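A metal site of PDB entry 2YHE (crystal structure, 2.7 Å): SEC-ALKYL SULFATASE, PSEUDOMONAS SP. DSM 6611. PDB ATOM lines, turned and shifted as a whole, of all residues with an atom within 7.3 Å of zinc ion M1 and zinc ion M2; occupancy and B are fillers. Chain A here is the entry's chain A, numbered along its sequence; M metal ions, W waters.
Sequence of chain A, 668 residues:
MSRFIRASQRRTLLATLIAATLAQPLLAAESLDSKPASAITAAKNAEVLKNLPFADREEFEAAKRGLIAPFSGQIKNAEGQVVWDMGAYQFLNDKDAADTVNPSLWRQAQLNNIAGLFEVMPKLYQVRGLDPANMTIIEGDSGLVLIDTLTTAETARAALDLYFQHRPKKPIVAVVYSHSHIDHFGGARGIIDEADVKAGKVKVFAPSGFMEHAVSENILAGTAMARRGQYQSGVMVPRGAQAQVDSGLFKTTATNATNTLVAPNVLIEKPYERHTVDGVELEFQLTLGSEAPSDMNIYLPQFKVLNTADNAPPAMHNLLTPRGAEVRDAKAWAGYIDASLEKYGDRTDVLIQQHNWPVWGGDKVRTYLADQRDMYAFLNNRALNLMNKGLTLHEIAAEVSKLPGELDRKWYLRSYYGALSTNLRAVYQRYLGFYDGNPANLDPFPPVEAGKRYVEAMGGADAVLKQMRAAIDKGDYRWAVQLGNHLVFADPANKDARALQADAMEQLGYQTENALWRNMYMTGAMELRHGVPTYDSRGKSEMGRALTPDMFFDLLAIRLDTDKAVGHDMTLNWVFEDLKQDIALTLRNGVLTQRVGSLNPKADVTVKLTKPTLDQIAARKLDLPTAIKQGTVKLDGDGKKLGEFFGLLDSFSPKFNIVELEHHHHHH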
ATOM      1  N   PRO A 132      -1.481 -15.766  28.391  1.00  0.00           N
ATOM      2  CA  PRO A 132      -0.077 -15.654  28.823  1.00  0.00           C
ATOM      3  C   PRO A 132       0.300 -14.218  29.280  1.00  0.00           C
ATOM      4  O   PRO A 132       0.991 -14.040  30.293  1.00  0.00           O
ATOM      5  CB  PRO A 132       0.726 -16.031  27.582  1.00  0.00           C
ATOM      6  CG  PRO A 132      -0.179 -16.910  26.826  1.00  0.00           C
ATOM      7  CD  PRO A 132      -1.556 -16.407  27.067  1.00  0.00           C
ATOM      8  N   ALA A 133      -0.207 -13.197  28.571  1.00  0.00           N
ATOM      9  CA  ALA A 133       0.053 -11.786  28.867  1.00  0.00           C
ATOM     10  C   ALA A 133      -1.105 -11.103  29.648  1.00  0.00           C
ATOM     11  O   ALA A 133      -2.152 -11.695  29.852  1.00  0.00           O
ATOM     12  CB  ALA A 133       0.327 -11.045  27.565  1.00  0.00           C
ATOM     13  N   ASN A 134      -0.897  -9.856  30.072  1.00  0.00           N
ATOM     14  CA  ASN A 134      -1.889  -9.032  30.759  1.00  0.00           C
ATOM     15  C   ASN A 134      -2.442  -7.992  29.776  1.00  0.00           C
ATOM     16  O   ASN A 134      -1.811  -7.687  28.754  1.00  0.00           O
ATOM     17  CB  ASN A 134      -1.250  -8.280  31.951  1.00  0.00           C
ATOM     18  CG  ASN A 134      -0.695  -9.153  33.051  1.00  0.00           C
ATOM     19  OD1 ASN A 134      -1.073 -10.311  33.218  1.00  0.00           O
ATOM     20  ND2 ASN A 134       0.189  -8.573  33.842  1.00  0.00           N
ATOM     21  N   ASP A 148      -1.952  -3.188  25.104  1.00  0.00           N
ATOM     22  CA  ASP A 148      -1.920  -4.574  24.620  1.00  0.00           C
ATOM     23  C   ASP A 148      -3.288  -5.232  24.525  1.00  0.00           C
ATOM     24  O   ASP A 148      -4.231  -4.818  25.199  1.00  0.00           O
ATOM     25  CB  ASP A 148      -0.805  -5.427  25.240  1.00  0.00           C
ATOM     26  CG  ASP A 148       0.602  -4.864  25.056  1.00  0.00           C
ATOM     27  OD1 ASP A 148       0.856  -4.244  24.012  1.00  0.00           O
ATOM     28  OD2 ASP A 148       1.448  -5.105  25.925  1.00  0.00           O
ATOM     29  N   SER A 178       2.793  -2.566  23.101  1.00  0.00           N
ATOM     30  CA  SER A 178       4.048  -2.266  23.828  1.00  0.00           C
ATOM     31  C   SER A 178       5.289  -2.831  23.111  1.00  0.00           C
ATOM     32  O   SER A 178       6.367  -2.229  23.166  1.00  0.00           O
ATOM     33  CB  SER A 178       3.965  -2.716  25.277  1.00  0.00           C
ATOM     34  OG  SER A 178       3.990  -4.118  25.425  1.00  0.00           O
ATOM     35  N   HIS A 179       5.116  -3.948  22.391  1.00  0.00           N
ATOM     36  CA  HIS A 179       6.155  -4.608  21.618  1.00  0.00           C
ATOM     37  C   HIS A 179       5.639  -5.619  20.588  1.00  0.00           C
ATOM     38  O   HIS A 179       4.450  -5.964  20.602  1.00  0.00           O
ATOM     39  CB  HIS A 179       7.220  -5.249  22.513  1.00  0.00           C
ATOM     40  CG  HIS A 179       6.704  -6.301  23.458  1.00  0.00           C
ATOM     41  ND1 HIS A 179       5.873  -5.977  24.524  1.00  0.00           N
ATOM     42  CD2 HIS A 179       7.038  -7.607  23.535  1.00  0.00           C
ATOM     43  CE1 HIS A 179       5.707  -7.098  25.183  1.00  0.00           C
ATOM     44  NE2 HIS A 179       6.390  -8.105  24.619  1.00  0.00           N
ATOM     45  N   SER A 180       6.560  -6.083  19.689  1.00  0.00           N
ATOM     46  CA  SER A 180       6.304  -7.007  18.567  1.00  0.00           C
ATOM     47  C   SER A 180       6.139  -8.468  18.941  1.00  0.00           C
ATOM     48  O   SER A 180       6.509  -9.357  18.169  1.00  0.00           O
ATOM     49  CB  SER A 180       7.343  -6.807  17.479  1.00  0.00           C
ATOM     50  OG  SER A 180       8.681  -6.942  17.963  1.00  0.00           O
ATOM     51  N   HIS A 181       5.565  -8.742  20.127  1.00  0.00           N
ATOM     52  CA  HIS A 181       5.311 -10.106  20.606  1.00  0.00           C
ATOM     53  C   HIS A 181       3.838 -10.491  20.479  1.00  0.00           C
ATOM     54  O   HIS A 181       2.971  -9.692  20.857  1.00  0.00           O
ATOM     55  CB  HIS A 181       5.872 -10.331  22.006  1.00  0.00           C
ATOM     56  CG  HIS A 181       7.377 -10.527  22.031  1.00  0.00           C
ATOM     57  ND1 HIS A 181       8.079 -10.598  23.223  1.00  0.00           N
ATOM     58  CD2 HIS A 181       8.247 -10.647  21.003  1.00  0.00           C
ATOM     59  CE1 HIS A 181       9.346 -10.778  22.879  1.00  0.00           C
ATOM     60  NE2 HIS A 181       9.490 -10.816  21.546  1.00  0.00           N
ATOM     61  N   ILE A 182       3.564 -11.680  19.914  1.00  0.00           N
ATOM     62  CA  ILE A 182       2.218 -12.234  19.692  1.00  0.00           C
ATOM     63  C   ILE A 182       1.295 -12.139  20.873  1.00  0.00           C
ATOM     64  O   ILE A 182       0.103 -11.902  20.669  1.00  0.00           O
ATOM     65  CB  ILE A 182       2.134 -13.658  19.097  1.00  0.00           C
ATOM     66  CG1 ILE A 182       2.979 -14.725  19.818  1.00  0.00           C
ATOM     67  CG2 ILE A 182       2.161 -13.707  17.627  1.00  0.00           C
ATOM     68  CD1 ILE A 182       2.149 -16.178  19.973  1.00  0.00           C
ATOM     69  N   ASP A 183       1.818 -12.274  22.114  1.00  0.00           N
ATOM     70  CA  ASP A 183       1.020 -12.197  23.341  1.00  0.00           C
ATOM     71  C   ASP A 183       0.523 -10.765  23.678  1.00  0.00           C
ATOM     72  O   ASP A 183      -0.166 -10.558  24.685  1.00  0.00           O
ATOM     73  CB  ASP A 183       1.727 -12.890  24.511  1.00  0.00           C
ATOM     74  CG  ASP A 183       3.167 -12.485  24.773  1.00  0.00           C
ATOM     75  OD1 ASP A 183       3.926 -12.300  23.793  1.00  0.00           O
ATOM     76  OD2 ASP A 183       3.544 -12.357  25.962  1.00  0.00           O
ATOM     77  N   HIS A 184       0.834  -9.791  22.806  1.00  0.00           N
ATOM     78  CA  HIS A 184       0.523  -8.387  23.009  1.00  0.00           C
ATOM     79  C   HIS A 184      -0.275  -7.787  21.874  1.00  0.00           C
ATOM     80  O   HIS A 184      -1.190  -6.999  22.126  1.00  0.00           O
ATOM     81  CB  HIS A 184       1.832  -7.614  23.322  1.00  0.00           C
ATOM     82  CG  HIS A 184       2.535  -8.179  24.524  1.00  0.00           C
ATOM     83  ND1 HIS A 184       2.287  -7.684  25.800  1.00  0.00           N
ATOM     84  CD2 HIS A 184       3.331  -9.265  24.616  1.00  0.00           C
ATOM     85  CE1 HIS A 184       2.983  -8.457  26.624  1.00  0.00           C
ATOM     86  NE2 HIS A 184       3.621  -9.433  25.967  1.00  0.00           N
ATOM     87  N   LEU A 249       6.194 -16.737  33.660  1.00  0.00           N
ATOM     88  CA  LEU A 249       5.560 -15.423  33.464  1.00  0.00           C
ATOM     89  C   LEU A 249       4.082 -15.560  33.192  1.00  0.00           C
ATOM     90  O   LEU A 249       3.369 -14.566  33.058  1.00  0.00           O
ATOM     91  CB  LEU A 249       6.249 -14.636  32.334  1.00  0.00           C
ATOM     92  CG  LEU A 249       7.724 -14.249  32.534  1.00  0.00           C
ATOM     93  CD1 LEU A 249       8.182 -13.372  31.410  1.00  0.00           C
ATOM     94  CD2 LEU A 249       7.982 -13.589  33.892  1.00  0.00           C
ATOM     95  N   PHE A 250       3.622 -16.816  33.070  1.00  0.00           N
ATOM     96  CA  PHE A 250       2.231 -17.196  32.770  1.00  0.00           C
ATOM     97  C   PHE A 250       2.078 -18.675  33.017  1.00  0.00           C
ATOM     98  O   PHE A 250       3.070 -19.349  33.381  1.00  0.00           O
ATOM     99  CB  PHE A 250       1.876 -16.876  31.312  1.00  0.00           C
ATOM    100  CG  PHE A 250       2.873 -17.307  30.255  1.00  0.00           C
ATOM    101  CD1 PHE A 250       3.916 -16.479  29.882  1.00  0.00           C
ATOM    102  CD2 PHE A 250       2.735 -18.525  29.620  1.00  0.00           C
ATOM    103  CE1 PHE A 250       4.845 -16.884  28.915  1.00  0.00           C
ATOM    104  CE2 PHE A 250       3.660 -18.945  28.670  1.00  0.00           C
ATOM    105  CZ  PHE A 250       4.710 -18.116  28.329  1.00  0.00           C
ATOM    106  N   GLU A 291      14.018  -6.586  25.178  1.00  0.00           N
ATOM    107  CA  GLU A 291      13.110  -7.740  25.271  1.00  0.00           C
ATOM    108  C   GLU A 291      12.527  -8.202  23.911  1.00  0.00           C
ATOM    109  O   GLU A 291      12.241  -9.386  23.710  1.00  0.00           O
ATOM    110  CB  GLU A 291      12.002  -7.494  26.325  1.00  0.00           C
ATOM    111  CG  GLU A 291      11.245  -8.750  26.719  1.00  0.00           C
ATOM    112  CD  GLU A 291       9.958  -8.970  25.944  1.00  0.00           C
ATOM    113  OE1 GLU A 291       9.507  -8.018  25.268  1.00  0.00           O
ATOM    114  OE2 GLU A 291       9.370 -10.070  26.071  1.00  0.00           O
ATOM    115  N   ALA A 292      12.357  -7.271  22.992  1.00  0.00           N
ATOM    116  CA  ALA A 292      11.833  -7.539  21.660  1.00  0.00           C
ATOM    117  C   ALA A 292      12.524  -6.532  20.722  1.00  0.00           C
ATOM    118  O   ALA A 292      12.927  -5.444  21.178  1.00  0.00           O
ATOM    119  CB  ALA A 292      10.304  -7.361  21.637  1.00  0.00           C
ATOM    120  N   ASP A 295      10.160  -2.489  20.702  1.00  0.00           N
ATOM    121  CA  ASP A 295       9.762  -2.514  22.114  1.00  0.00           C
ATOM    122  C   ASP A 295       9.789  -1.141  22.771  1.00  0.00           C
ATOM    123  O   ASP A 295      10.601  -0.294  22.396  1.00  0.00           O
ATOM    124  CB  ASP A 295      10.713  -3.482  22.846  1.00  0.00           C
ATOM    125  CG  ASP A 295      10.484  -3.750  24.307  1.00  0.00           C
ATOM    126  OD1 ASP A 295       9.334  -3.570  24.785  1.00  0.00           O
ATOM    127  OD2 ASP A 295      11.443  -4.203  24.983  1.00  0.00           O
ATOM    128  N   ALA A 309       6.220  -2.844  30.264  1.00  0.00           N
ATOM    129  CA  ALA A 309       5.900  -3.879  29.271  1.00  0.00           C
ATOM    130  C   ALA A 309       6.429  -5.242  29.771  1.00  0.00           C
ATOM    131  O   ALA A 309       5.998  -5.668  30.836  1.00  0.00           O
ATOM    132  CB  ALA A 309       6.490  -3.514  27.902  1.00  0.00           C
ATOM    133  N   ASP A 310       7.383  -5.875  29.054  1.00  0.00           N
ATOM    134  CA  ASP A 310       7.999  -7.150  29.455  1.00  0.00           C
ATOM    135  C   ASP A 310       9.488  -6.934  29.739  1.00  0.00           C
ATOM    136  O   ASP A 310      10.257  -7.893  29.796  1.00  0.00           O
ATOM    137  CB  ASP A 310       7.822  -8.251  28.374  1.00  0.00           C
ATOM    138  CG  ASP A 310       6.402  -8.664  28.019  1.00  0.00           C
ATOM    139  OD1 ASP A 310       5.448  -8.009  28.503  1.00  0.00           O
ATOM    140  OD2 ASP A 310       6.253  -9.620  27.230  1.00  0.00           O
ATOM    141  N   ASN A 311       9.878  -5.679  29.933  1.00  0.00           N
ATOM    142  CA  ASN A 311      11.253  -5.265  30.155  1.00  0.00           C
ATOM    143  C   ASN A 311      11.794  -5.502  31.529  1.00  0.00           C
ATOM    144  O   ASN A 311      12.998  -5.570  31.684  1.00  0.00           O
ATOM    145  CB  ASN A 311      11.443  -3.821  29.717  1.00  0.00           C
ATOM    146  CG  ASN A 311      11.172  -3.625  28.251  1.00  0.00           C
ATOM    147  OD1 ASN A 311      11.722  -4.337  27.396  1.00  0.00           O
ATOM    148  ND2 ASN A 311      10.286  -2.696  27.938  1.00  0.00           N
ATOM    149  N   HIS A 317      14.314 -12.759  32.531  1.00  0.00           N
ATOM    150  CA  HIS A 317      13.720 -13.001  31.215  1.00  0.00           C
ATOM    151  C   HIS A 317      14.754 -13.672  30.292  1.00  0.00           C
ATOM    152  O   HIS A 317      15.899 -13.919  30.705  1.00  0.00           O
ATOM    153  CB  HIS A 317      13.171 -11.697  30.634  1.00  0.00           C
ATOM    154  CG  HIS A 317      12.033 -11.831  29.665  1.00  0.00           C
ATOM    155  ND1 HIS A 317      11.939 -12.893  28.784  1.00  0.00           N
ATOM    156  CD2 HIS A 317      11.028 -10.966  29.410  1.00  0.00           C
ATOM    157  CE1 HIS A 317      10.888 -12.638  28.032  1.00  0.00           C
ATOM    158  NE2 HIS A 317      10.290 -11.502  28.392  1.00  0.00           N
ATOM    159  N   ARG A 323      11.624 -20.764  21.948  1.00  0.00           N
ATOM    160  CA  ARG A 323      10.812 -20.885  20.742  1.00  0.00           C
ATOM    161  C   ARG A 323      11.561 -20.457  19.489  1.00  0.00           C
ATOM    162  O   ARG A 323      11.208 -20.882  18.384  1.00  0.00           O
ATOM    163  CB  ARG A 323       9.510 -20.113  20.886  1.00  0.00           C
ATOM    164  CG  ARG A 323       9.672 -18.611  21.012  1.00  0.00           C
ATOM    165  CD  ARG A 323       8.397 -17.942  21.479  1.00  0.00           C
ATOM    166  NE  ARG A 323       8.664 -16.553  21.854  1.00  0.00           N
ATOM    167  CZ  ARG A 323       8.714 -15.525  21.017  1.00  0.00           C
ATOM    168  NH1 ARG A 323       8.525 -15.716  19.706  1.00  0.00           N
ATOM    169  NH2 ARG A 323       8.966 -14.310  21.460  1.00  0.00           N
ATOM    170  N   ARG A 328      18.860 -11.056  22.083  1.00  0.00           N
ATOM    171  CA  ARG A 328      18.536  -9.830  22.750  1.00  0.00           C
ATOM    172  C   ARG A 328      19.796  -9.228  23.325  1.00  0.00           C
ATOM    173  O   ARG A 328      20.757  -9.945  23.631  1.00  0.00           O
ATOM    174  CB  ARG A 328      17.436 -10.118  23.805  1.00  0.00           C
ATOM    175  CG  ARG A 328      16.163 -10.578  23.097  1.00  0.00           C
ATOM    176  CD  ARG A 328      15.177 -11.247  23.969  1.00  0.00           C
ATOM    177  NE  ARG A 328      14.006 -11.699  23.186  1.00  0.00           N
ATOM    178  CZ  ARG A 328      13.004 -12.431  23.684  1.00  0.00           C
ATOM    179  NH1 ARG A 328      12.998 -12.774  24.974  1.00  0.00           N
ATOM    180  NH2 ARG A 328      12.000 -12.791  22.909  1.00  0.00           N
ATOM    181  N   GLN A 354       3.224  -6.134  31.671  1.00  0.00           N
ATOM    182  CA  GLN A 354       2.362  -6.859  30.753  1.00  0.00           C
ATOM    183  C   GLN A 354       2.388  -8.403  30.960  1.00  0.00           C
ATOM    184  O   GLN A 354       1.789  -9.161  30.190  1.00  0.00           O
ATOM    185  CB  GLN A 354       2.551  -6.382  29.307  1.00  0.00           C
ATOM    186  CG  GLN A 354       2.177  -4.902  29.112  1.00  0.00           C
ATOM    187  CD  GLN A 354       0.739  -4.585  29.452  1.00  0.00           C
ATOM    188  OE1 GLN A 354       0.424  -4.079  30.532  1.00  0.00           O
ATOM    189  NE2 GLN A 354      -0.164  -4.867  28.535  1.00  0.00           N
ATOM    190  N   HIS A 355       3.045  -8.828  32.054  1.00  0.00           N
ATOM    191  CA  HIS A 355       3.089 -10.179  32.615  1.00  0.00           C
ATOM    192  C   HIS A 355       3.197  -9.974  34.105  1.00  0.00           C
ATOM    193  O   HIS A 355       3.875  -9.039  34.535  1.00  0.00           O
ATOM    194  CB  HIS A 355       4.298 -11.007  32.150  1.00  0.00           C
ATOM    195  CG  HIS A 355       4.186 -11.448  30.725  1.00  0.00           C
ATOM    196  ND1 HIS A 355       3.414 -12.544  30.353  1.00  0.00           N
ATOM    197  CD2 HIS A 355       4.751 -10.911  29.615  1.00  0.00           C
ATOM    198  CE1 HIS A 355       3.549 -12.628  29.038  1.00  0.00           C
ATOM    199  NE2 HIS A 355       4.340 -11.675  28.551  1.00  0.00           N
ATOM    200  N   TYR A 417      11.972 -18.098  34.180  1.00  0.00           N
ATOM    201  CA  TYR A 417      11.686 -17.955  32.761  1.00  0.00           C
ATOM    202  C   TYR A 417      13.014 -18.061  32.007  1.00  0.00           C
ATOM    203  O   TYR A 417      13.314 -19.111  31.433  1.00  0.00           O
ATOM    204  CB  TYR A 417      10.971 -16.614  32.506  1.00  0.00           C
ATOM    205  CG  TYR A 417      10.181 -16.591  31.226  1.00  0.00           C
ATOM    206  CD1 TYR A 417       8.956 -17.248  31.134  1.00  0.00           C
ATOM    207  CD2 TYR A 417      10.622 -15.874  30.122  1.00  0.00           C
ATOM    208  CE1 TYR A 417       8.213 -17.237  29.952  1.00  0.00           C
ATOM    209  CE2 TYR A 417       9.900 -15.871  28.920  1.00  0.00           C
ATOM    210  CZ  TYR A 417       8.698 -16.565  28.843  1.00  0.00           C
ATOM    211  OH  TYR A 417       7.941 -16.543  27.703  1.00  0.00           O
HETATM  212 ZN    ZN M   1       4.674 -10.915  26.699  1.00  0.00          ZN
HETATM  213 ZN    ZN M   2       7.455  -9.938  25.212  1.00  0.00          ZN
HETATM  214  O   HOH W   1       6.570 -12.115  26.051  1.00  0.00           O
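A ring nitrogen (ND1) of His 184 lies within hydrogen-bond range of the side-chain carboxylate (OD2) of Asp 148. A ring nitrogen (ND1) of His 355 sits at hydrogen-bond distance from the backbone carbonyl oxygen of Pro 132, 2.8 Å away. ND1 of His 355 sits at hydrogen-bond distance from O of Leu 249, at 3.4 Å. ND2 of Asn 134 lies close to N of His 355 (3.4 Å). The side-chain carboxylate (OE2) of Glu 291 sits close to a ring nitrogen (NE2) of His 317 (2.9 Å). O of Glu 291 sits at hydrogen-bond distance from NE of Arg 328, at 3.0 Å. The guanidinium group (NH2) of Arg 328 lies close to a ring nitrogen (NE2) of His 181 (3.5 Å). ND1 of His 179 sits at hydrogen-bond distance from OG of Ser 178 (2.8 Å).
Five residues have an atom within 4 Å of zinc ion M1: His 179, Asp 183, His 184, Asp 310 and His 355. The nearest printed residue that does not touch zinc ion M1 is Ala 133 (4.4 Å).
The nearest printed residue that does not touch zinc ion M2 is Asp 183 (4.5 Å).
NE2 of His 184 is bound to zinc ion M1, 2.0 Å away. Zinc ion M1 is bound by OD2 of Asp 183, 2.0 Å away. NE2 of His 355 is bound to zinc ion M1, 2.0 Å away. OD2 of Asp 310 binds zinc ion M1, at 2.1 Å. Zinc ion M1 is bound by water W1 (2.3 Å).
Zinc ion M2 is bound by OE2 of Glu 291, at 2.1 Å. Zinc ion M2 is bound by ND1 of His 181, 2.2 Å away. Zinc ion M2 is bound by a ring nitrogen (NE2) of His 179, 2.2 Å away. OD2 of Asp 310 is bound to zinc ion M2, 2.4 Å away. Water W1 binds zinc ion M2 (2.5 Å). Slightly farther from zinc ion M2 lies the side-chain carboxylate (OE1) of Glu 291 (2.8 Å).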
